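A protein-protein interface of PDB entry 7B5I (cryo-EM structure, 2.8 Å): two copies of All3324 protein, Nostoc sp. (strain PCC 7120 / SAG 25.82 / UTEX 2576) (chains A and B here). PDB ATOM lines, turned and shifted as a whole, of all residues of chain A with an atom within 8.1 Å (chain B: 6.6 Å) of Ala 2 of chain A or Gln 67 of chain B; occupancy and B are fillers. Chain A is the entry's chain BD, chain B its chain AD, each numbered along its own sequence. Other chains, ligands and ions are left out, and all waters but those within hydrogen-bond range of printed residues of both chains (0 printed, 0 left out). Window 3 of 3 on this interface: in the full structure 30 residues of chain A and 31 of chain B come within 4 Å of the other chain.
Ala 2 of chain A touches just one residue of chain B: Gln 67. Gln 67 of chain B touches just these residues of chain A: Ala 2 (3.5 Å) and Val 101 (3.5 Å). Of the printed residues of chain A, Thr 65 of chain B touches Pro 5 (3.6 Å) and Leu 6 (3.2 Å). Printed residues of chain A within 4 Å of Gly 68 of chain B: Asn 142 (3.1 Å). Of the printed residues of chain B, Asn 142 of chain A touches Phe 66, Gly 68 and Asp 69. The nearest residue of chain B that does not touch Ala 2 of chain A is Phe 66 of chain B (4.6 Å). The nearest printed residue of chain A that does not touch Asp 69 of chain B is Gly 143 of chain A (5.6 Å).
No position is printed for both chains.
Among the printed residues, pairs that only touch across the chains: Ala 2 of chain A with Gln 67 of chain B, Glu 3 of chain A with Phe 66 of chain B, Tyr 4 of chain A with Phe 66 of chain B, Pro 5 of chain A with Thr 65 of chain B, Pro 5 of chain A with Phe 66 of chain B and Val 101 of chain A with Gln 67 of chain B.
Of the 12 printed residues of chain A, 7 touch a printed residue of chain B. Of the 6 printed residues of chain B, 5 touch a printed residue of chain A. Hydrophobic or aromatic side chains of chain B within 4 Å of the printed part of chain A: Phe 66. Among the printed residues, 10 pairs touch across the chains.
O of Phe 66 of chain B is in hydrogen-bond range of ND2 of Asn 142 of chain A, at 3.2 Å. The backbone carbonyl oxygen of Thr 65 of chain B lies within hydrogen-bond range of the backbone NH of Leu 6 of chain A (3.2 Å). OD1 of Asn 142 of chain A sits at hydrogen-bond distance from N of Gly 68 of chain B (3.1 Å). O of Asp 69 of chain B sits at hydrogen-bond distance from ND2 of Asn 142 of chain A (2.7 Å).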
ATOM      1  N   ALA A   2       5.118  22.828  15.142  1.00  0.00           N
ATOM      2  CA  ALA A   2       6.217  22.299  15.937  1.00  0.00           C
ATOM      3  C   ALA A   2       7.059  23.423  16.533  1.00  0.00           C
ATOM      4  O   ALA A   2       7.706  23.247  17.565  1.00  0.00           O
ATOM      5  CB  ALA A   2       7.083  21.374  15.095  1.00  0.00           C
ATOM      6  N   GLU A   3       7.045  24.577  15.875  1.00  0.00           N
ATOM      7  CA  GLU A   3       7.807  25.732  16.336  1.00  0.00           C
ATOM      8  C   GLU A   3       6.883  26.859  16.783  1.00  0.00           C
ATOM      9  O   GLU A   3       7.274  27.719  17.573  1.00  0.00           O
ATOM     10  CB  GLU A   3       8.747  26.228  15.237  1.00  0.00           C
ATOM     11  CG  GLU A   3       9.574  27.441  15.629  1.00  0.00           C
ATOM     12  CD  GLU A   3      10.475  27.919  14.506  1.00  0.00           C
ATOM     13  OE1 GLU A   3      11.174  28.937  14.695  1.00  0.00           O
ATOM     14  OE2 GLU A   3      10.484  27.278  13.434  1.00  0.00           O
ATOM     15  N   TYR A   4       5.656  26.850  16.272  1.00  0.00           N
ATOM     16  CA  TYR A   4       4.677  27.871  16.616  1.00  0.00           C
ATOM     17  C   TYR A   4       3.890  27.427  17.838  1.00  0.00           C
ATOM     18  O   TYR A   4       3.717  26.224  18.060  1.00  0.00           O
ATOM     19  CB  TYR A   4       3.678  28.132  15.483  1.00  0.00           C
ATOM     20  CG  TYR A   4       4.213  28.839  14.268  1.00  0.00           C
ATOM     21  CD1 TYR A   4       5.367  29.605  14.330  1.00  0.00           C
ATOM     22  CD2 TYR A   4       3.523  28.785  13.064  1.00  0.00           C
ATOM     23  CE1 TYR A   4       5.843  30.260  13.208  1.00  0.00           C
ATOM     24  CE2 TYR A   4       3.983  29.437  11.948  1.00  0.00           C
ATOM     25  CZ  TYR A   4       5.140  30.174  12.018  1.00  0.00           C
ATOM     26  OH  TYR A   4       5.595  30.827  10.895  1.00  0.00           O
ATOM     27  N   PRO A   5       3.401  28.361  18.643  1.00  0.00           N
ATOM     28  CA  PRO A   5       2.452  27.995  19.696  1.00  0.00           C
ATOM     29  C   PRO A   5       1.086  27.702  19.094  1.00  0.00           C
ATOM     30  O   PRO A   5       0.730  28.203  18.028  1.00  0.00           O
ATOM     31  CB  PRO A   5       2.413  29.228  20.606  1.00  0.00           C
ATOM     32  CG  PRO A   5       3.176  30.295  19.910  1.00  0.00           C
ATOM     33  CD  PRO A   5       3.725  29.794  18.626  1.00  0.00           C
ATOM     34  N   LEU A   6       0.323  26.873  19.789  1.00  0.00           N
ATOM     35  CA  LEU A   6      -0.943  26.390  19.258  1.00  0.00           C
ATOM     36  C   LEU A   6      -2.101  27.301  19.650  1.00  0.00           C
ATOM     37  O   LEU A   6      -2.072  27.941  20.702  1.00  0.00           O
ATOM     38  CB  LEU A   6      -1.223  24.981  19.764  1.00  0.00           C
ATOM     39  CG  LEU A   6      -0.245  23.869  19.414  1.00  0.00           C
ATOM     40  CD1 LEU A   6      -0.488  22.665  20.297  1.00  0.00           C
ATOM     41  CD2 LEU A   6      -0.392  23.496  17.961  1.00  0.00           C
ATOM     42  N   ASN A  95      -4.535  20.382  15.047  1.00  0.00           N
ATOM     43  CA  ASN A  95      -3.874  21.495  14.410  1.00  0.00           C
ATOM     44  C   ASN A  95      -4.390  21.699  12.991  1.00  0.00           C
ATOM     45  O   ASN A  95      -5.237  20.957  12.545  1.00  0.00           O
ATOM     46  CB  ASN A  95      -2.362  21.329  14.374  1.00  0.00           C
ATOM     47  CG  ASN A  95      -1.909  20.272  13.432  1.00  0.00           C
ATOM     48  OD1 ASN A  95      -2.668  19.788  12.642  1.00  0.00           O
ATOM     49  ND2 ASN A  95      -0.644  19.972  13.473  1.00  0.00           N
ATOM     50  N   GLU A  99      -4.485  16.904  12.839  1.00  0.00           N
ATOM     51  CA  GLU A  99      -3.801  15.780  13.464  1.00  0.00           C
ATOM     52  C   GLU A  99      -3.851  15.964  14.972  1.00  0.00           C
ATOM     53  O   GLU A  99      -3.547  17.051  15.468  1.00  0.00           O
ATOM     54  CB  GLU A  99      -2.352  15.698  12.986  1.00  0.00           C
ATOM     55  CG  GLU A  99      -2.203  15.538  11.482  1.00  0.00           C
ATOM     56  CD  GLU A  99      -0.755  15.467  11.042  1.00  0.00           C
ATOM     57  OE1 GLU A  99       0.136  15.536  11.914  1.00  0.00           O
ATOM     58  OE2 GLU A  99      -0.506  15.342   9.824  1.00  0.00           O
ATOM     59  N   PRO A 100      -4.284  14.924  15.700  1.00  0.00           N
ATOM     60  CA  PRO A 100      -4.377  14.988  17.161  1.00  0.00           C
ATOM     61  C   PRO A 100      -3.014  15.323  17.739  1.00  0.00           C
ATOM     62  O   PRO A 100      -2.050  14.612  17.457  1.00  0.00           O
ATOM     63  CB  PRO A 100      -4.789  13.563  17.556  1.00  0.00           C
ATOM     64  CG  PRO A 100      -4.462  12.712  16.372  1.00  0.00           C
ATOM     65  CD  PRO A 100      -4.658  13.599  15.180  1.00  0.00           C
ATOM     66  N   VAL A 101      -2.925  16.386  18.533  1.00  0.00           N
ATOM     67  CA  VAL A 101      -1.631  16.760  19.084  1.00  0.00           C
ATOM     68  C   VAL A 101      -1.591  16.549  20.589  1.00  0.00           C
ATOM     69  O   VAL A 101      -0.655  15.936  21.110  1.00  0.00           O
ATOM     70  CB  VAL A 101      -1.283  18.218  18.731  1.00  0.00           C
ATOM     71  CG1 VAL A 101       0.100  18.559  19.233  1.00  0.00           C
ATOM     72  CG2 VAL A 101      -1.357  18.425  17.250  1.00  0.00           C
ATOM     73  N   VAL A 102      -2.599  17.040  21.300  1.00  0.00           N
ATOM     74  CA  VAL A 102      -2.697  16.867  22.740  1.00  0.00           C
ATOM     75  C   VAL A 102      -3.969  16.092  23.027  1.00  0.00           C
ATOM     76  O   VAL A 102      -5.037  16.429  22.502  1.00  0.00           O
ATOM     77  CB  VAL A 102      -2.695  18.212  23.489  1.00  0.00           C
ATOM     78  CG1 VAL A 102      -2.720  17.981  24.984  1.00  0.00           C
ATOM     79  CG2 VAL A 102      -1.486  19.024  23.105  1.00  0.00           C
ATOM     80  N   ASN A 142       1.058  14.395  25.272  1.00  0.00           N
ATOM     81  CA  ASN A 142       1.528  15.364  24.290  1.00  0.00           C
ATOM     82  C   ASN A 142       2.789  14.826  23.634  1.00  0.00           C
ATOM     83  O   ASN A 142       3.786  14.569  24.314  1.00  0.00           O
ATOM     84  CB  ASN A 142       1.806  16.720  24.935  1.00  0.00           C
ATOM     85  CG  ASN A 142       2.201  17.778  23.925  1.00  0.00           C
ATOM     86  OD1 ASN A 142       2.365  17.497  22.744  1.00  0.00           O
ATOM     87  ND2 ASN A 142       2.362  19.005  24.391  1.00  0.00           N
ATOM     88  N   GLY A 143       2.751  14.679  22.317  1.00  0.00           N
ATOM     89  CA  GLY A 143       3.906  14.227  21.571  1.00  0.00           C
ATOM     90  C   GLY A 143       4.286  12.800  21.891  1.00  0.00           C
ATOM     91  O   GLY A 143       3.553  12.103  22.588  1.00  0.00           O
ATOM     92  N   ARG B  19      12.615  23.043  27.859  1.00  0.00           N
ATOM     93  CA  ARG B  19      12.449  24.341  27.203  1.00  0.00           C
ATOM     94  C   ARG B  19      12.398  25.544  28.147  1.00  0.00           C
ATOM     95  O   ARG B  19      12.392  25.397  29.370  1.00  0.00           O
ATOM     96  CB  ARG B  19      11.199  24.329  26.318  1.00  0.00           C
ATOM     97  CG  ARG B  19      11.256  23.336  25.169  1.00  0.00           C
ATOM     98  CD  ARG B  19      12.346  23.704  24.176  1.00  0.00           C
ATOM     99  NE  ARG B  19      12.379  22.789  23.039  1.00  0.00           N
ATOM    100  CZ  ARG B  19      13.209  22.907  22.008  1.00  0.00           C
ATOM    101  NH1 ARG B  19      14.080  23.906  21.967  1.00  0.00           N
ATOM    102  NH2 ARG B  19      13.168  22.028  21.016  1.00  0.00           N
ATOM    103  N   THR B  65       1.632  26.668  24.973  1.00  0.00           N
ATOM    104  CA  THR B  65       1.663  25.246  24.654  1.00  0.00           C
ATOM    105  C   THR B  65       2.248  24.993  23.269  1.00  0.00           C
ATOM    106  O   THR B  65       1.855  25.629  22.289  1.00  0.00           O
ATOM    107  CB  THR B  65       0.256  24.654  24.726  1.00  0.00           C
ATOM    108  OG1 THR B  65      -0.400  25.120  25.908  1.00  0.00           O
ATOM    109  CG2 THR B  65       0.325  23.143  24.758  1.00  0.00           C
ATOM    110  N   PHE B  66       3.162  24.027  23.191  1.00  0.00           N
ATOM    111  CA  PHE B  66       3.832  23.667  21.950  1.00  0.00           C
ATOM    112  C   PHE B  66       3.706  22.173  21.708  1.00  0.00           C
ATOM    113  O   PHE B  66       3.564  21.392  22.648  1.00  0.00           O
ATOM    114  CB  PHE B  66       5.318  24.055  21.982  1.00  0.00           C
ATOM    115  CG  PHE B  66       5.565  25.532  21.918  1.00  0.00           C
ATOM    116  CD1 PHE B  66       5.290  26.337  22.999  1.00  0.00           C
ATOM    117  CD2 PHE B  66       6.107  26.109  20.786  1.00  0.00           C
ATOM    118  CE1 PHE B  66       5.521  27.687  22.950  1.00  0.00           C
ATOM    119  CE2 PHE B  66       6.346  27.465  20.735  1.00  0.00           C
ATOM    120  CZ  PHE B  66       6.051  28.253  21.820  1.00  0.00           C
ATOM    121  N   GLN B  67       3.735  21.794  20.436  1.00  0.00           N
ATOM    122  CA  GLN B  67       3.692  20.386  20.071  1.00  0.00           C
ATOM    123  C   GLN B  67       4.970  19.672  20.493  1.00  0.00           C
ATOM    124  O   GLN B  67       6.077  20.124  20.191  1.00  0.00           O
ATOM    125  CB  GLN B  67       3.491  20.234  18.567  1.00  0.00           C
ATOM    126  CG  GLN B  67       3.413  18.794  18.112  1.00  0.00           C
ATOM    127  CD  GLN B  67       3.601  18.643  16.619  1.00  0.00           C
ATOM    128  OE1 GLN B  67       4.413  19.338  16.009  1.00  0.00           O
ATOM    129  NE2 GLN B  67       2.851  17.728  16.018  1.00  0.00           N
ATOM    130  N   GLY B  68       4.814  18.548  21.183  1.00  0.00           N
ATOM    131  CA  GLY B  68       5.932  17.736  21.608  1.00  0.00           C
ATOM    132  C   GLY B  68       6.446  18.001  23.004  1.00  0.00           C
ATOM    133  O   GLY B  68       7.307  17.252  23.472  1.00  0.00           O
ATOM    134  N   ASP B  69       5.946  19.027  23.687  1.00  0.00           N
ATOM    135  CA  ASP B  69       6.457  19.429  24.993  1.00  0.00           C
ATOM    136  C   ASP B  69       5.443  19.038  26.060  1.00  0.00           C
ATOM    137  O   ASP B  69       4.332  19.574  26.096  1.00  0.00           O
ATOM    138  CB  ASP B  69       6.736  20.928  25.022  1.00  0.00           C
ATOM    139  CG  ASP B  69       7.822  21.296  26.003  1.00  0.00           C
ATOM    140  OD1 ASP B  69       9.007  21.175  25.641  1.00  0.00           O
ATOM    141  OD2 ASP B  69       7.498  21.710  27.131  1.00  0.00           O
